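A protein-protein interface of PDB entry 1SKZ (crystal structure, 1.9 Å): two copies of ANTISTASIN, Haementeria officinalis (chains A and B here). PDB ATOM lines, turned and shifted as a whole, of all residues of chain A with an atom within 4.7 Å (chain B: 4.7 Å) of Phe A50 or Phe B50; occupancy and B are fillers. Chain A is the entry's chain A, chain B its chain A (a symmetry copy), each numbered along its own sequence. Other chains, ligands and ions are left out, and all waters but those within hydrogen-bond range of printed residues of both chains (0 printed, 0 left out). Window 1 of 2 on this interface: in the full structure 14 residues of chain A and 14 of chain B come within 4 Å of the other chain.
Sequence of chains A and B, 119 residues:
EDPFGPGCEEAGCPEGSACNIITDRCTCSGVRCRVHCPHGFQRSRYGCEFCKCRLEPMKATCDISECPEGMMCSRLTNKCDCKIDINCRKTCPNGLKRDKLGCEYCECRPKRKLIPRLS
Of the printed residues of chain B, Gln A42 touches Gln B42 (2.7 Å) and Lys B52 (3.5 Å).
Cys A48 touches none of the printed residues of chain B.
Phe A50 touches just one residue of chain B: Phe B50.
Phe B50 touches just one residue of chain A: Phe A50 (3.0 Å).
Of the printed residues of chain A, Cys B51 touches Ser A44 (3.2 Å).
Of the printed residues of chain A, Lys B52 touches Gln A42.
The nearest residue of chain B that does not touch Phe A50 is Arg B32 (4.2 Å).
The nearest printed residue of chain A that does not touch Cys B51 is Phe A50 (4.9 Å).
The side-chain amide oxygen (OE1) of Gln B42 lies close to the side-chain amide oxygen (OE1) of Gln A42 (2.7 Å).
The guanidinium group (NH2) of Arg A32 lies close to the guanidinium group (NH2) of Arg B32.
Among the printed residues, pairs that only touch across the chains: Phe A50 with Phe B50 (3.0 Å), Ser A44 with Cys B51 (3.2 Å), Cys A51 with Ser B44 (3.2 Å), Gln A42 with Lys B52 (3.5 Å) and Lys A52 with Gln B42 (3.5 Å).
Arg A32 touches its own counterpart, Arg B32.
Gln A42 touches its own counterpart, Gln B42.
Gln A42 touches Lys B52, and with the chains exchanged Lys A52 touches Gln B42.
Ser A44 touches Cys B51, and with the chains exchanged Cys A51 touches Ser B44.
Of the 7 pairs that touch across the chains among the printed residues, 7 have their exchanged pair printed and touching as well.
The backbone NH (N) of Gln A42 lies within hydrogen-bond range of the backbone carbonyl oxygen (O) of Lys A52, at 2.9 Å.
O of Gln A42 is in hydrogen-bond range of N of Phe A50, 3.1 Å away.
N of Cys A48 is in hydrogen-bond range of OG of Ser A44.
N of Phe B50 lies within hydrogen-bond range of O of Gln B42, at 3.1 Å.
The backbone carbonyl oxygen (O) of Lys B52 is in hydrogen-bond range of the backbone NH (N) of Gln B42 (2.9 Å).
OG of Ser B44 lies within hydrogen-bond range of N of Cys B48 (3.2 Å).
Printed residues of chain A that touch a printed residue of chain B: Arg A32, Gln A42, Ser A44, Phe A50, Cys A51 and Lys A52.
Hydrophobic or aromatic side chains of chain A within 4 Å of the printed part of chain B: Phe A50.
Of the 10 printed residues of chain B, 6 touch a printed residue of chain A.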
ATOM      1  N   VAL A  31      30.157  16.853 -21.008  1.00  0.00           N
ATOM      2  CA  VAL A  31      29.943  18.103 -20.294  1.00  0.00           C
ATOM      3  C   VAL A  31      31.319  18.736 -20.003  1.00  0.00           C
ATOM      4  O   VAL A  31      32.240  18.052 -19.565  1.00  0.00           O
ATOM      5  CB  VAL A  31      29.171  17.805 -18.976  1.00  0.00           C
ATOM      6  CG1 VAL A  31      29.002  19.060 -18.139  1.00  0.00           C
ATOM      7  CG2 VAL A  31      27.828  17.178 -19.312  1.00  0.00           C
ATOM      8  N   ARG A  32      31.496  20.010 -20.338  1.00  0.00           N
ATOM      9  CA  ARG A  32      32.829  20.595 -20.192  1.00  0.00           C
ATOM     10  C   ARG A  32      32.908  21.255 -18.832  1.00  0.00           C
ATOM     11  O   ARG A  32      33.410  22.355 -18.718  1.00  0.00           O
ATOM     12  CB  ARG A  32      33.138  21.655 -21.272  1.00  0.00           C
ATOM     13  CG  ARG A  32      33.188  21.178 -22.711  1.00  0.00           C
ATOM     14  CD  ARG A  32      31.765  20.986 -23.186  1.00  0.00           C
ATOM     15  NE  ARG A  32      31.519  21.161 -24.622  1.00  0.00           N
ATOM     16  CZ  ARG A  32      31.952  20.343 -25.583  1.00  0.00           C
ATOM     17  NH1 ARG A  32      33.055  19.599 -25.402  1.00  0.00           N
ATOM     18  NH2 ARG A  32      31.413  20.432 -26.793  1.00  0.00           N
ATOM     19  N   PHE A  41      22.070  17.057 -15.779  1.00  0.00           N
ATOM     20  CA  PHE A  41      22.315  17.979 -16.881  1.00  0.00           C
ATOM     21  C   PHE A  41      21.223  17.917 -17.920  1.00  0.00           C
ATOM     22  O   PHE A  41      20.645  16.876 -18.160  1.00  0.00           O
ATOM     23  CB  PHE A  41      23.647  17.631 -17.562  1.00  0.00           C
ATOM     24  CG  PHE A  41      24.856  17.891 -16.705  1.00  0.00           C
ATOM     25  CD1 PHE A  41      25.168  19.190 -16.278  1.00  0.00           C
ATOM     26  CD2 PHE A  41      25.690  16.841 -16.313  1.00  0.00           C
ATOM     27  CE1 PHE A  41      26.264  19.451 -15.484  1.00  0.00           C
ATOM     28  CE2 PHE A  41      26.814  17.104 -15.498  1.00  0.00           C
ATOM     29  CZ  PHE A  41      27.091  18.440 -15.086  1.00  0.00           C
ATOM     30  N   GLN A  42      20.910  19.065 -18.500  1.00  0.00           N
ATOM     31  CA  GLN A  42      20.047  19.155 -19.667  1.00  0.00           C
ATOM     32  C   GLN A  42      20.679  18.470 -20.849  1.00  0.00           C
ATOM     33  O   GLN A  42      21.888  18.266 -20.886  1.00  0.00           O
ATOM     34  CB  GLN A  42      19.752  20.625 -20.003  1.00  0.00           C
ATOM     35  CG  GLN A  42      19.019  21.267 -18.851  1.00  0.00           C
ATOM     36  CD  GLN A  42      18.318  22.549 -19.219  1.00  0.00           C
ATOM     37  OE1 GLN A  42      17.849  22.726 -20.355  1.00  0.00           O
ATOM     38  NE2 GLN A  42      18.263  23.479 -18.259  1.00  0.00           N
ATOM     39  N   SER A  44      20.674  18.255 -25.260  1.00  0.00           N
ATOM     40  CA  SER A  44      20.138  18.610 -26.570  1.00  0.00           C
ATOM     41  C   SER A  44      19.061  17.612 -26.997  1.00  0.00           C
ATOM     42  O   SER A  44      18.963  16.491 -26.463  1.00  0.00           O
ATOM     43  CB  SER A  44      21.259  18.651 -27.619  1.00  0.00           C
ATOM     44  OG  SER A  44      21.854  17.378 -27.754  1.00  0.00           O
ATOM     45  N   CYS A  48      22.610  14.661 -26.307  1.00  0.00           N
ATOM     46  CA  CYS A  48      23.841  14.961 -25.563  1.00  0.00           C
ATOM     47  C   CYS A  48      23.685  15.948 -24.383  1.00  0.00           C
ATOM     48  O   CYS A  48      23.085  17.020 -24.520  1.00  0.00           O
ATOM     49  CB  CYS A  48      24.920  15.497 -26.527  1.00  0.00           C
ATOM     50  SG  CYS A  48      25.358  14.337 -27.857  1.00  0.00           S
ATOM     51  N   GLU A  49      24.242  15.567 -23.234  1.00  0.00           N
ATOM     52  CA  GLU A  49      24.348  16.444 -22.052  1.00  0.00           C
ATOM     53  C   GLU A  49      25.223  17.682 -22.289  1.00  0.00           C
ATOM     54  O   GLU A  49      26.234  17.633 -23.016  1.00  0.00           O
ATOM     55  CB  GLU A  49      24.898  15.663 -20.838  1.00  0.00           C
ATOM     56  CG  GLU A  49      23.851  14.780 -20.191  1.00  0.00           C
ATOM     57  CD  GLU A  49      24.336  14.047 -18.958  1.00  0.00           C
ATOM     58  OE1 GLU A  49      25.545  13.836 -18.852  1.00  0.00           O
ATOM     59  OE2 GLU A  49      23.497  13.665 -18.100  1.00  0.00           O
ATOM     60  N   PHE A  50      24.828  18.783 -21.671  1.00  0.00           N
ATOM     61  CA  PHE A  50      25.650  19.963 -21.671  1.00  0.00           C
ATOM     62  C   PHE A  50      25.538  20.554 -20.292  1.00  0.00           C
ATOM     63  O   PHE A  50      24.618  20.189 -19.537  1.00  0.00           O
ATOM     64  CB  PHE A  50      25.179  20.940 -22.747  1.00  0.00           C
ATOM     65  CG  PHE A  50      25.396  20.426 -24.117  1.00  0.00           C
ATOM     66  CD1 PHE A  50      26.701  20.221 -24.586  1.00  0.00           C
ATOM     67  CD2 PHE A  50      24.317  19.929 -24.866  1.00  0.00           C
ATOM     68  CE1 PHE A  50      26.937  19.504 -25.776  1.00  0.00           C
ATOM     69  CE2 PHE A  50      24.524  19.227 -26.052  1.00  0.00           C
ATOM     70  CZ  PHE A  50      25.833  19.007 -26.516  1.00  0.00           C
ATOM     71  N   CYS A  51      26.444  21.498 -19.987  1.00  0.00           N
ATOM     72  CA  CYS A  51      26.594  22.010 -18.622  1.00  0.00           C
ATOM     73  C   CYS A  51      25.560  23.080 -18.262  1.00  0.00           C
ATOM     74  O   CYS A  51      25.897  24.253 -18.026  1.00  0.00           O
ATOM     75  CB  CYS A  51      28.012  22.569 -18.400  1.00  0.00           C
ATOM     76  SG  CYS A  51      28.314  22.941 -16.652  1.00  0.00           S
ATOM     77  N   LYS A  52      24.310  22.660 -18.151  1.00  0.00           N
ATOM     78  CA  LYS A  52      23.242  23.488 -17.600  1.00  0.00           C
ATOM     79  C   LYS A  52      22.389  22.495 -16.799  1.00  0.00           C
ATOM     80  O   LYS A  52      22.013  21.444 -17.343  1.00  0.00           O
ATOM     81  CB  LYS A  52      22.393  24.087 -18.751  1.00  0.00           C
ATOM     82  CG  LYS A  52      21.254  25.035 -18.280  1.00  0.00           C
ATOM     83  CD  LYS A  52      20.535  25.750 -19.443  1.00  0.00           C
ATOM     84  CE  LYS A  52      19.997  27.112 -18.991  1.00  0.00           C
ATOM     85  NZ  LYS A  52      21.171  28.144 -19.012  1.00  0.00           N
ATOM     86  N   VAL B  31      26.689  24.727 -32.065  1.00  0.00           N
ATOM     87  CA  VAL B  31      25.496  23.893 -32.041  1.00  0.00           C
ATOM     88  C   VAL B  31      25.642  22.810 -33.130  1.00  0.00           C
ATOM     89  O   VAL B  31      26.032  23.106 -34.256  1.00  0.00           O
ATOM     90  CB  VAL B  31      24.250  24.788 -32.301  1.00  0.00           C
ATOM     91  CG1 VAL B  31      22.981  23.959 -32.385  1.00  0.00           C
ATOM     92  CG2 VAL B  31      24.152  25.841 -31.209  1.00  0.00           C
ATOM     93  N   ARG B  32      25.429  21.547 -32.776  1.00  0.00           N
ATOM     94  CA  ARG B  32      25.686  20.491 -33.756  1.00  0.00           C
ATOM     95  C   ARG B  32      24.389  20.192 -34.478  1.00  0.00           C
ATOM     96  O   ARG B  32      24.059  19.041 -34.682  1.00  0.00           O
ATOM     97  CB  ARG B  32      26.201  19.187 -33.108  1.00  0.00           C
ATOM     98  CG  ARG B  32      27.539  19.254 -32.397  1.00  0.00           C
ATOM     99  CD  ARG B  32      27.323  19.931 -31.062  1.00  0.00           C
ATOM    100  NE  ARG B  32      28.237  19.559 -29.977  1.00  0.00           N
ATOM    101  CZ  ARG B  32      29.535  19.865 -29.923  1.00  0.00           C
ATOM    102  NH1 ARG B  32      30.234  20.075 -31.050  1.00  0.00           N
ATOM    103  NH2 ARG B  32      30.175  19.745 -28.766  1.00  0.00           N
ATOM    104  N   PHE B  41      18.790  29.251 -28.912  1.00  0.00           N
ATOM    105  CA  PHE B  41      19.353  28.090 -28.233  1.00  0.00           C
ATOM    106  C   PHE B  41      19.669  28.381 -26.787  1.00  0.00           C
ATOM    107  O   PHE B  41      20.035  29.486 -26.436  1.00  0.00           O
ATOM    108  CB  PHE B  41      20.652  27.660 -28.931  1.00  0.00           C
ATOM    109  CG  PHE B  41      20.445  27.104 -30.314  1.00  0.00           C
ATOM    110  CD1 PHE B  41      19.698  25.933 -30.513  1.00  0.00           C
ATOM    111  CD2 PHE B  41      20.989  27.746 -31.429  1.00  0.00           C
ATOM    112  CE1 PHE B  41      19.486  25.411 -31.771  1.00  0.00           C
ATOM    113  CE2 PHE B  41      20.774  27.215 -32.720  1.00  0.00           C
ATOM    114  CZ  PHE B  41      20.006  26.024 -32.875  1.00  0.00           C
ATOM    115  N   GLN B  42      19.470  27.385 -25.939  1.00  0.00           N
ATOM    116  CA  GLN B  42      19.926  27.416 -24.558  1.00  0.00           C
ATOM    117  C   GLN B  42      21.429  27.469 -24.495  1.00  0.00           C
ATOM    118  O   GLN B  42      22.111  27.114 -25.450  1.00  0.00           O
ATOM    119  CB  GLN B  42      19.408  26.186 -23.797  1.00  0.00           C
ATOM    120  CG  GLN B  42      17.900  26.207 -23.773  1.00  0.00           C
ATOM    121  CD  GLN B  42      17.298  25.310 -22.722  1.00  0.00           C
ATOM    122  OE1 GLN B  42      17.876  25.101 -21.643  1.00  0.00           O
ATOM    123  NE2 GLN B  42      16.130  24.742 -23.040  1.00  0.00           N
ATOM    124  N   SER B  44      24.915  26.655 -21.910  1.00  0.00           N
ATOM    125  CA  SER B  44      25.518  26.279 -20.635  1.00  0.00           C
ATOM    126  C   SER B  44      25.776  27.520 -19.779  1.00  0.00           C
ATOM    127  O   SER B  44      25.807  28.661 -20.277  1.00  0.00           O
ATOM    128  CB  SER B  44      26.833  25.519 -20.864  1.00  0.00           C
ATOM    129  OG  SER B  44      27.768  26.339 -21.531  1.00  0.00           O
ATOM    130  N   CYS B  48      28.188  28.708 -23.594  1.00  0.00           N
ATOM    131  CA  CYS B  48      28.060  28.082 -24.918  1.00  0.00           C
ATOM    132  C   CYS B  48      26.651  27.557 -25.275  1.00  0.00           C
ATOM    133  O   CYS B  48      26.010  26.853 -24.489  1.00  0.00           O
ATOM    134  CB  CYS B  48      29.075  26.926 -25.051  1.00  0.00           C
ATOM    135  SG  CYS B  48      30.807  27.445 -24.859  1.00  0.00           S
ATOM    136  N   GLU B  49      26.192  27.909 -26.477  1.00  0.00           N
ATOM    137  CA  GLU B  49      24.952  27.368 -27.064  1.00  0.00           C
ATOM    138  C   GLU B  49      25.006  25.855 -27.314  1.00  0.00           C
ATOM    139  O   GLU B  49      26.060  25.293 -27.670  1.00  0.00           O
ATOM    140  CB  GLU B  49      24.613  28.087 -28.388  1.00  0.00           C
ATOM    141  CG  GLU B  49      24.008  29.458 -28.170  1.00  0.00           C
ATOM    142  CD  GLU B  49      23.605  30.167 -29.446  1.00  0.00           C
ATOM    143  OE1 GLU B  49      24.181  29.850 -30.487  1.00  0.00           O
ATOM    144  OE2 GLU B  49      22.717  31.059 -29.398  1.00  0.00           O
ATOM    145  N   PHE B  50      23.867  25.207 -27.128  1.00  0.00           N
ATOM    146  CA  PHE B  50      23.739  23.822 -27.492  1.00  0.00           C
ATOM    147  C   PHE B  50      22.369  23.670 -28.094  1.00  0.00           C
ATOM    148  O   PHE B  50      21.516  24.560 -27.919  1.00  0.00           O
ATOM    149  CB  PHE B  50      23.923  22.930 -26.265  1.00  0.00           C
ATOM    150  CG  PHE B  50      25.302  22.973 -25.733  1.00  0.00           C
ATOM    151  CD1 PHE B  50      26.363  22.478 -26.504  1.00  0.00           C
ATOM    152  CD2 PHE B  50      25.590  23.704 -24.568  1.00  0.00           C
ATOM    153  CE1 PHE B  50      27.700  22.729 -26.139  1.00  0.00           C
ATOM    154  CE2 PHE B  50      26.905  23.956 -24.180  1.00  0.00           C
ATOM    155  CZ  PHE B  50      27.970  23.473 -24.961  1.00  0.00           C
ATOM    156  N   CYS B  51      22.148  22.523 -28.758  1.00  0.00           N
ATOM    157  CA  CYS B  51      20.945  22.323 -29.571  1.00  0.00           C
ATOM    158  C   CYS B  51      19.720  21.921 -28.746  1.00  0.00           C
ATOM    159  O   CYS B  51      19.186  20.806 -28.879  1.00  0.00           O
ATOM    160  CB  CYS B  51      21.196  21.270 -30.668  1.00  0.00           C
ATOM    161  SG  CYS B  51      19.830  21.213 -31.858  1.00  0.00           S
ATOM    162  N   LYS B  52      19.231  22.855 -27.946  1.00  0.00           N
ATOM    163  CA  LYS B  52      17.949  22.723 -27.263  1.00  0.00           C
ATOM    164  C   LYS B  52      17.364  24.141 -27.311  1.00  0.00           C
ATOM    165  O   LYS B  52      18.063  25.096 -26.937  1.00  0.00           O
ATOM    166  CB  LYS B  52      18.177  22.307 -25.788  1.00  0.00           C
ATOM    167  CG  LYS B  52      16.870  22.083 -24.976  1.00  0.00           C
ATOM    168  CD  LYS B  52      17.118  21.507 -23.566  1.00  0.00           C
ATOM    169  CE  LYS B  52      15.928  20.656 -23.111  1.00  0.00           C
ATOM    170  NZ  LYS B  52      16.044  19.242 -23.768  1.00  0.00           N
